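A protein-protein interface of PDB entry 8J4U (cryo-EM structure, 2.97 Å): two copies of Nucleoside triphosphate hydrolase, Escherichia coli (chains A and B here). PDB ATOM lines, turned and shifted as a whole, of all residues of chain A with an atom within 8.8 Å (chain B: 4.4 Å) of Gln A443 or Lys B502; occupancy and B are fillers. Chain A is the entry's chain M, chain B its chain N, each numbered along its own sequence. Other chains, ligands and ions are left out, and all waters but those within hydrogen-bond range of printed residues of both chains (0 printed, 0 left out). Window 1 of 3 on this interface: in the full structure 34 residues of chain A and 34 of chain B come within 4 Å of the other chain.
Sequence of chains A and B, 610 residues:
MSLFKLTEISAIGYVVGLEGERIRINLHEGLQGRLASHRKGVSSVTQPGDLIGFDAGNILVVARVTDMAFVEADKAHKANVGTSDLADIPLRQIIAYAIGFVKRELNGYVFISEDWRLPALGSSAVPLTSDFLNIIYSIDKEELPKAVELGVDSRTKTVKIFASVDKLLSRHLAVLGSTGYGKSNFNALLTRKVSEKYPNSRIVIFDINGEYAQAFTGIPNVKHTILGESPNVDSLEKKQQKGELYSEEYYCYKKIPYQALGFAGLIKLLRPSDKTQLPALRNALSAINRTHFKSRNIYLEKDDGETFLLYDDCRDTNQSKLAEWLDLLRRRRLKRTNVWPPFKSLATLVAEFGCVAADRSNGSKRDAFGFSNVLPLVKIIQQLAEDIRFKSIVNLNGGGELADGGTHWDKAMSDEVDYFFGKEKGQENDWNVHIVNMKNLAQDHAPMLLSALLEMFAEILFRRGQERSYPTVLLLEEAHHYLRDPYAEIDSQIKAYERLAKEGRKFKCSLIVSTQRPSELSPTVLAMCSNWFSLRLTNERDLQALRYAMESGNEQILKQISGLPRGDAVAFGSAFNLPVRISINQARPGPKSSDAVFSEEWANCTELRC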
ATOM      1  N   ILE A 208      -6.251 -21.304  26.169  1.00  0.00           N
ATOM      2  CA  ILE A 208      -5.120 -20.446  26.521  1.00  0.00           C
ATOM      3  C   ILE A 208      -4.950 -20.258  28.019  1.00  0.00           C
ATOM      4  O   ILE A 208      -3.986 -19.607  28.441  1.00  0.00           O
ATOM      5  CB  ILE A 208      -5.266 -19.051  25.879  1.00  0.00           C
ATOM      6  CG1 ILE A 208      -5.626 -19.157  24.396  1.00  0.00           C
ATOM      7  CG2 ILE A 208      -3.989 -18.252  26.035  1.00  0.00           C
ATOM      8  CD1 ILE A 208      -4.570 -19.804  23.544  1.00  0.00           C
ATOM      9  N   ASN A 209      -5.841 -20.814  28.840  1.00  0.00           N
ATOM     10  CA  ASN A 209      -5.816 -20.537  30.273  1.00  0.00           C
ATOM     11  C   ASN A 209      -5.944 -21.764  31.163  1.00  0.00           C
ATOM     12  O   ASN A 209      -5.753 -21.627  32.374  1.00  0.00           O
ATOM     13  CB  ASN A 209      -6.938 -19.553  30.639  1.00  0.00           C
ATOM     14  CG  ASN A 209      -6.936 -18.315  29.767  1.00  0.00           C
ATOM     15  OD1 ASN A 209      -7.484 -18.316  28.666  1.00  0.00           O
ATOM     16  ND2 ASN A 209      -6.323 -17.247  30.260  1.00  0.00           N
ATOM     17  N   ARG A 389      12.498 -19.383  27.307  1.00  0.00           N
ATOM     18  CA  ARG A 389      11.051 -19.271  27.199  1.00  0.00           C
ATOM     19  C   ARG A 389      10.520 -19.720  25.844  1.00  0.00           C
ATOM     20  O   ARG A 389       9.317 -19.600  25.594  1.00  0.00           O
ATOM     21  CB  ARG A 389      10.636 -17.820  27.465  1.00  0.00           C
ATOM     22  CG  ARG A 389       9.176 -17.619  27.802  1.00  0.00           C
ATOM     23  CD  ARG A 389       8.940 -17.551  29.298  1.00  0.00           C
ATOM     24  NE  ARG A 389       7.633 -16.968  29.601  1.00  0.00           N
ATOM     25  CZ  ARG A 389       6.635 -17.594  30.218  1.00  0.00           C
ATOM     26  NH1 ARG A 389       6.751 -18.854  30.612  1.00  0.00           N
ATOM     27  NH2 ARG A 389       5.498 -16.950  30.434  1.00  0.00           N
ATOM     28  N   ASN A 440       1.758 -22.155  29.333  1.00  0.00           N
ATOM     29  CA  ASN A 440       3.174 -21.845  29.411  1.00  0.00           C
ATOM     30  C   ASN A 440       3.657 -21.043  28.213  1.00  0.00           C
ATOM     31  O   ASN A 440       4.840 -20.695  28.160  1.00  0.00           O
ATOM     32  CB  ASN A 440       3.990 -23.138  29.526  1.00  0.00           C
ATOM     33  CG  ASN A 440       3.803 -23.824  30.860  1.00  0.00           C
ATOM     34  OD1 ASN A 440       3.342 -23.216  31.825  1.00  0.00           O
ATOM     35  ND2 ASN A 440       4.153 -25.102  30.923  1.00  0.00           N
ATOM     36  N   LEU A 441       2.786 -20.743  27.257  1.00  0.00           N
ATOM     37  CA  LEU A 441       3.125 -19.943  26.093  1.00  0.00           C
ATOM     38  C   LEU A 441       3.040 -18.461  26.438  1.00  0.00           C
ATOM     39  O   LEU A 441       2.314 -18.056  27.348  1.00  0.00           O
ATOM     40  CB  LEU A 441       2.184 -20.276  24.935  1.00  0.00           C
ATOM     41  CG  LEU A 441       2.348 -19.510  23.623  1.00  0.00           C
ATOM     42  CD1 LEU A 441       3.650 -19.869  22.947  1.00  0.00           C
ATOM     43  CD2 LEU A 441       1.179 -19.793  22.707  1.00  0.00           C
ATOM     44  N   ALA A 442       3.792 -17.654  25.695  1.00  0.00           N
ATOM     45  CA  ALA A 442       3.921 -16.229  25.960  1.00  0.00           C
ATOM     46  C   ALA A 442       3.193 -15.417  24.898  1.00  0.00           C
ATOM     47  O   ALA A 442       3.134 -15.814  23.728  1.00  0.00           O
ATOM     48  CB  ALA A 442       5.393 -15.822  26.009  1.00  0.00           C
ATOM     49  N   GLN A 443       2.639 -14.280  25.320  1.00  0.00           N
ATOM     50  CA  GLN A 443       1.924 -13.380  24.422  1.00  0.00           C
ATOM     51  C   GLN A 443       2.871 -12.734  23.418  1.00  0.00           C
ATOM     52  O   GLN A 443       2.429 -12.043  22.496  1.00  0.00           O
ATOM     53  CB  GLN A 443       1.198 -12.297  25.221  1.00  0.00           C
ATOM     54  CG  GLN A 443       0.080 -12.811  26.105  1.00  0.00           C
ATOM     55  CD  GLN A 443      -0.259 -11.850  27.226  1.00  0.00           C
ATOM     56  OE1 GLN A 443      -0.281 -10.635  27.030  1.00  0.00           O
ATOM     57  NE2 GLN A 443      -0.518 -12.390  28.411  1.00  0.00           N
ATOM     58  N   ASP A 444       4.174 -12.950  23.594  1.00  0.00           N
ATOM     59  CA  ASP A 444       5.168 -12.445  22.658  1.00  0.00           C
ATOM     60  C   ASP A 444       5.464 -13.431  21.538  1.00  0.00           C
ATOM     61  O   ASP A 444       5.825 -13.011  20.433  1.00  0.00           O
ATOM     62  CB  ASP A 444       6.467 -12.120  23.400  1.00  0.00           C
ATOM     63  CG  ASP A 444       6.229 -11.341  24.678  1.00  0.00           C
ATOM     64  OD1 ASP A 444       6.202 -11.966  25.759  1.00  0.00           O
ATOM     65  OD2 ASP A 444       6.070 -10.105  24.603  1.00  0.00           O
ATOM     66  N   HIS A 445       5.318 -14.728  21.801  1.00  0.00           N
ATOM     67  CA  HIS A 445       5.584 -15.766  20.816  1.00  0.00           C
ATOM     68  C   HIS A 445       4.319 -16.394  20.245  1.00  0.00           C
ATOM     69  O   HIS A 445       4.411 -17.162  19.283  1.00  0.00           O
ATOM     70  CB  HIS A 445       6.452 -16.866  21.437  1.00  0.00           C
ATOM     71  CG  HIS A 445       7.808 -16.398  21.860  1.00  0.00           C
ATOM     72  ND1 HIS A 445       8.533 -15.473  21.141  1.00  0.00           N
ATOM     73  CD2 HIS A 445       8.569 -16.722  22.931  1.00  0.00           C
ATOM     74  CE1 HIS A 445       9.684 -15.248  21.750  1.00  0.00           C
ATOM     75  NE2 HIS A 445       9.730 -15.994  22.839  1.00  0.00           N
ATOM     76  N   ALA A 446       3.150 -16.095  20.808  1.00  0.00           N
ATOM     77  CA  ALA A 446       1.921 -16.713  20.312  1.00  0.00           C
ATOM     78  C   ALA A 446       1.632 -16.370  18.857  1.00  0.00           C
ATOM     79  O   ALA A 446       1.281 -17.283  18.088  1.00  0.00           O
ATOM     80  CB  ALA A 446       0.750 -16.316  21.213  1.00  0.00           C
ATOM     81  N   PRO A 447       1.748 -15.113  18.407  1.00  0.00           N
ATOM     82  CA  PRO A 447       1.379 -14.792  17.021  1.00  0.00           C
ATOM     83  C   PRO A 447       2.264 -15.453  15.977  1.00  0.00           C
ATOM     84  O   PRO A 447       1.988 -15.352  14.778  1.00  0.00           O
ATOM     85  CB  PRO A 447       1.514 -13.265  16.961  1.00  0.00           C
ATOM     86  CG  PRO A 447       1.540 -12.805  18.360  1.00  0.00           C
ATOM     87  CD  PRO A 447       2.105 -13.909  19.174  1.00  0.00           C
ATOM     88  N   MET A 448       3.325 -16.132  16.410  1.00  0.00           N
ATOM     89  CA  MET A 448       4.249 -16.791  15.499  1.00  0.00           C
ATOM     90  C   MET A 448       4.117 -18.302  15.497  1.00  0.00           C
ATOM     91  O   MET A 448       4.374 -18.929  14.468  1.00  0.00           O
ATOM     92  CB  MET A 448       5.695 -16.430  15.855  1.00  0.00           C
ATOM     93  CG  MET A 448       5.976 -14.946  15.881  1.00  0.00           C
ATOM     94  SD  MET A 448       7.734 -14.585  15.719  1.00  0.00           S
ATOM     95  CE  MET A 448       8.363 -15.303  17.233  1.00  0.00           C
ATOM     96  N   LEU A 450       1.144 -19.808  16.602  1.00  0.00           N
ATOM     97  CA  LEU A 450      -0.266 -20.109  16.407  1.00  0.00           C
ATOM     98  C   LEU A 450      -0.810 -19.562  15.096  1.00  0.00           C
ATOM     99  O   LEU A 450      -2.004 -19.726  14.823  1.00  0.00           O
ATOM    100  CB  LEU A 450      -1.096 -19.558  17.573  1.00  0.00           C
ATOM    101  CG  LEU A 450      -1.124 -20.421  18.832  1.00  0.00           C
ATOM    102  CD1 LEU A 450       0.211 -20.409  19.534  1.00  0.00           C
ATOM    103  CD2 LEU A 450      -2.213 -19.941  19.762  1.00  0.00           C
ATOM    104  N   GLU A 478      -9.630 -16.196  22.642  1.00  0.00           N
ATOM    105  CA  GLU A 478      -8.690 -15.074  22.676  1.00  0.00           C
ATOM    106  C   GLU A 478      -8.053 -14.872  21.300  1.00  0.00           C
ATOM    107  O   GLU A 478      -6.833 -14.803  21.159  1.00  0.00           O
ATOM    108  CB  GLU A 478      -7.624 -15.280  23.752  1.00  0.00           C
ATOM    109  CG  GLU A 478      -8.182 -15.343  25.162  1.00  0.00           C
ATOM    110  CD  GLU A 478      -8.769 -14.026  25.622  1.00  0.00           C
ATOM    111  OE1 GLU A 478      -8.262 -12.966  25.200  1.00  0.00           O
ATOM    112  OE2 GLU A 478      -9.741 -14.050  26.406  1.00  0.00           O
ATOM    113  N   HIS A 480      -7.993 -12.375  19.208  1.00  0.00           N
ATOM    114  CA  HIS A 480      -7.403 -11.109  18.794  1.00  0.00           C
ATOM    115  C   HIS A 480      -5.898 -11.069  19.009  1.00  0.00           C
ATOM    116  O   HIS A 480      -5.250 -10.123  18.551  1.00  0.00           O
ATOM    117  CB  HIS A 480      -8.068  -9.938  19.525  1.00  0.00           C
ATOM    118  CG  HIS A 480      -7.976 -10.009  21.017  1.00  0.00           C
ATOM    119  ND1 HIS A 480      -8.647 -10.954  21.763  1.00  0.00           N
ATOM    120  CD2 HIS A 480      -7.307  -9.237  21.904  1.00  0.00           C
ATOM    121  CE1 HIS A 480      -8.386 -10.767  23.044  1.00  0.00           C
ATOM    122  NE2 HIS A 480      -7.574  -9.732  23.157  1.00  0.00           N
ATOM    123  N   HIS A 481      -5.328 -12.069  19.686  1.00  0.00           N
ATOM    124  CA  HIS A 481      -3.880 -12.122  19.843  1.00  0.00           C
ATOM    125  C   HIS A 481      -3.198 -12.595  18.565  1.00  0.00           C
ATOM    126  O   HIS A 481      -2.107 -12.121  18.227  1.00  0.00           O
ATOM    127  CB  HIS A 481      -3.505 -13.043  21.003  1.00  0.00           C
ATOM    128  CG  HIS A 481      -3.920 -12.530  22.345  1.00  0.00           C
ATOM    129  ND1 HIS A 481      -4.323 -11.230  22.556  1.00  0.00           N
ATOM    130  CD2 HIS A 481      -3.987 -13.145  23.550  1.00  0.00           C
ATOM    131  CE1 HIS A 481      -4.626 -11.066  23.832  1.00  0.00           C
ATOM    132  NE2 HIS A 481      -4.430 -12.213  24.457  1.00  0.00           N
ATOM    133  N   TYR A 482      -3.826 -13.527  17.836  1.00  0.00           N
ATOM    134  CA  TYR A 482      -3.130 -14.221  16.758  1.00  0.00           C
ATOM    135  C   TYR A 482      -3.964 -14.374  15.489  1.00  0.00           C
ATOM    136  O   TYR A 482      -3.613 -15.188  14.627  1.00  0.00           O
ATOM    137  CB  TYR A 482      -2.671 -15.597  17.241  1.00  0.00           C
ATOM    138  CG  TYR A 482      -3.779 -16.471  17.771  1.00  0.00           C
ATOM    139  CD1 TYR A 482      -4.013 -16.580  19.135  1.00  0.00           C
ATOM    140  CD2 TYR A 482      -4.583 -17.201  16.911  1.00  0.00           C
ATOM    141  CE1 TYR A 482      -5.021 -17.383  19.622  1.00  0.00           C
ATOM    142  CE2 TYR A 482      -5.594 -18.005  17.390  1.00  0.00           C
ATOM    143  CZ  TYR A 482      -5.808 -18.092  18.746  1.00  0.00           C
ATOM    144  OH  TYR A 482      -6.811 -18.892  19.232  1.00  0.00           O
ATOM    145  N   GLU B 498       8.492  -5.788  28.548  1.00  0.00           N
ATOM    146  CA  GLU B 498       7.283  -5.592  29.343  1.00  0.00           C
ATOM    147  C   GLU B 498       6.587  -6.927  29.595  1.00  0.00           C
ATOM    148  O   GLU B 498       5.373  -7.061  29.448  1.00  0.00           O
ATOM    149  CB  GLU B 498       6.343  -4.608  28.652  1.00  0.00           C
ATOM    150  CG  GLU B 498       5.787  -5.098  27.330  1.00  0.00           C
ATOM    151  CD  GLU B 498       5.081  -4.005  26.557  1.00  0.00           C
ATOM    152  OE1 GLU B 498       5.123  -2.839  27.000  1.00  0.00           O
ATOM    153  OE2 GLU B 498       4.484  -4.312  25.505  1.00  0.00           O
ATOM    154  N   ARG B 499       7.359  -7.938  29.995  1.00  0.00           N
ATOM    155  CA  ARG B 499       6.771  -9.231  30.323  1.00  0.00           C
ATOM    156  C   ARG B 499       6.194  -9.277  31.729  1.00  0.00           C
ATOM    157  O   ARG B 499       5.363 -10.146  32.012  1.00  0.00           O
ATOM    158  CB  ARG B 499       7.806 -10.344  30.174  1.00  0.00           C
ATOM    159  CG  ARG B 499       7.986 -10.834  28.755  1.00  0.00           C
ATOM    160  CD  ARG B 499       8.945 -12.008  28.698  1.00  0.00           C
ATOM    161  NE  ARG B 499       9.094 -12.527  27.343  1.00  0.00           N
ATOM    162  CZ  ARG B 499      10.046 -13.373  26.968  1.00  0.00           C
ATOM    163  NH1 ARG B 499      10.944 -13.803  27.841  1.00  0.00           N
ATOM    164  NH2 ARG B 499      10.101 -13.790  25.713  1.00  0.00           N
ATOM    165  N   LEU B 500       6.616  -8.377  32.618  1.00  0.00           N
ATOM    166  CA  LEU B 500       6.117  -8.409  33.986  1.00  0.00           C
ATOM    167  C   LEU B 500       4.691  -7.891  34.088  1.00  0.00           C
ATOM    168  O   LEU B 500       3.989  -8.227  35.047  1.00  0.00           O
ATOM    169  CB  LEU B 500       7.035  -7.599  34.901  1.00  0.00           C
ATOM    170  CG  LEU B 500       6.897  -7.871  36.398  1.00  0.00           C
ATOM    171  CD1 LEU B 500       7.193  -9.319  36.713  1.00  0.00           C
ATOM    172  CD2 LEU B 500       7.812  -6.967  37.181  1.00  0.00           C
ATOM    173  N   ALA B 501       4.247  -7.089  33.123  1.00  0.00           N
ATOM    174  CA  ALA B 501       2.872  -6.616  33.111  1.00  0.00           C
ATOM    175  C   ALA B 501       1.918  -7.617  32.478  1.00  0.00           C
ATOM    176  O   ALA B 501       0.703  -7.500  32.667  1.00  0.00           O
ATOM    177  CB  ALA B 501       2.779  -5.284  32.368  1.00  0.00           C
ATOM    178  N   LYS B 502       2.437  -8.590  31.734  1.00  0.00           N
ATOM    179  CA  LYS B 502       1.621  -9.606  31.084  1.00  0.00           C
ATOM    180  C   LYS B 502       1.622 -10.927  31.841  1.00  0.00           C
ATOM    181  O   LYS B 502       0.556 -11.441  32.187  1.00  0.00           O
ATOM    182  CB  LYS B 502       2.113  -9.824  29.649  1.00  0.00           C
ATOM    183  CG  LYS B 502       2.225  -8.545  28.844  1.00  0.00           C
ATOM    184  CD  LYS B 502       2.846  -8.791  27.484  1.00  0.00           C
ATOM    185  CE  LYS B 502       2.293  -7.829  26.446  1.00  0.00           C
ATOM    186  NZ  LYS B 502       3.212  -7.669  25.289  1.00  0.00           N
ATOM    187  N   GLU B 503       2.797 -11.490  32.105  1.00  0.00           N
ATOM    188  CA  GLU B 503       2.909 -12.746  32.843  1.00  0.00           C
ATOM    189  C   GLU B 503       3.088 -12.495  34.338  1.00  0.00           C
ATOM    190  O   GLU B 503       4.012 -13.006  34.964  1.00  0.00           O
ATOM    191  CB  GLU B 503       4.071 -13.562  32.288  1.00  0.00           C
ATOM    192  CG  GLU B 503       3.956 -13.910  30.807  1.00  0.00           C
ATOM    193  CD  GLU B 503       2.984 -15.043  30.543  1.00  0.00           C
ATOM    194  OE1 GLU B 503       2.954 -16.001  31.343  1.00  0.00           O
ATOM    195  OE2 GLU B 503       2.250 -14.975  29.533  1.00  0.00           O
ATOM    196  N   GLY B 504       2.199 -11.692  34.917  1.00  0.00           N
ATOM    197  CA  GLY B 504       2.264 -11.388  36.335  1.00  0.00           C
ATOM    198  C   GLY B 504       1.144 -12.016  37.136  1.00  0.00           C
ATOM    199  O   GLY B 504       1.345 -12.445  38.277  1.00  0.00           O
ATOM    200  N   MET B 528      -4.381  -3.608  30.467  1.00  0.00           N
ATOM    201  CA  MET B 528      -4.342  -4.706  31.422  1.00  0.00           C
ATOM    202  C   MET B 528      -4.758  -4.282  32.828  1.00  0.00           C
ATOM    203  O   MET B 528      -4.477  -5.009  33.788  1.00  0.00           O
ATOM    204  CB  MET B 528      -2.937  -5.309  31.458  1.00  0.00           C
ATOM    205  CG  MET B 528      -2.560  -6.074  30.205  1.00  0.00           C
ATOM    206  SD  MET B 528      -3.243  -7.740  30.181  1.00  0.00           S
ATOM    207  CE  MET B 528      -2.282  -8.504  31.481  1.00  0.00           C
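OD2 of Asp A444 is in salt-bridge range of NZ of Lys B502 (3.8 Å). The guanidinium group (NH2) of Arg A389 is in salt-bridge range of the side-chain carboxylate (OE1) of Glu B503 (2.9 Å). The guanidinium group (NE) of Arg B499 lies within salt-bridge range of the side-chain carboxylate (OD1) of Asp A444 (3.3 Å).
The side-chain amino group (NZ) of Lys B502 lies within salt-bridge range of the side-chain carboxylate (OE2) of Glu B498, 3.6 Å away.
Among the printed residues, merely in contact across the chains: Leu A441 with Glu B503 (3.8 Å), Gln A443 with Lys B502 (3.6 Å), Gln A443 with Glu B503 (3.95 Å) and His A445 with Arg B499 (3.6 Å).
Ile A208 touches none of the printed residues of chain B. Gln A443 touches two residues of chain B. Printed residues of chain B within 4 Å of Asp A444: Arg B499 and Lys B502. Met A448 touches none of the printed residues of chain B. Printed residues of chain A within 4 Å of Arg B499: Asp A444 (3.3 Å) and His A445 (3.6 Å). No residue of chain A comes within 4 Å of Ala B501. Of chain A, only Gln A443 and Asp A444 come within 4 Å of Lys B502. The nearest printed residue of chain B that does not touch Gln A443 is Met B528 (5.2 Å). The nearest residue of chain A that does not touch Lys B502 is Ala A442 (7.1 Å). The nearest printed residue of chain A that does not touch Glu B503 is Ala A442 (4.1 Å).
Of the 8 printed residues of chain B, 3 touch a printed residue of chain A. Printed residues of chain A that touch a printed residue of chain B: Arg A389, Leu A441, Gln A443, Asp A444 and His A445. Hydrophobic or aromatic side chains of chain A that line the printed part of chain B: His A445. Among the printed residues, Asp or Glu carboxylates within 4 Å of a Lys or Arg side-chain nitrogen of the other chain: Arg A389 with Glu B503, Asp A444 with Arg B499 and Asp A444 with Lys B502.
No position is printed for both chains. Of the 7 pairs that touch across the chains among the printed residues, none has its exchanged pair printed and touching as well.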
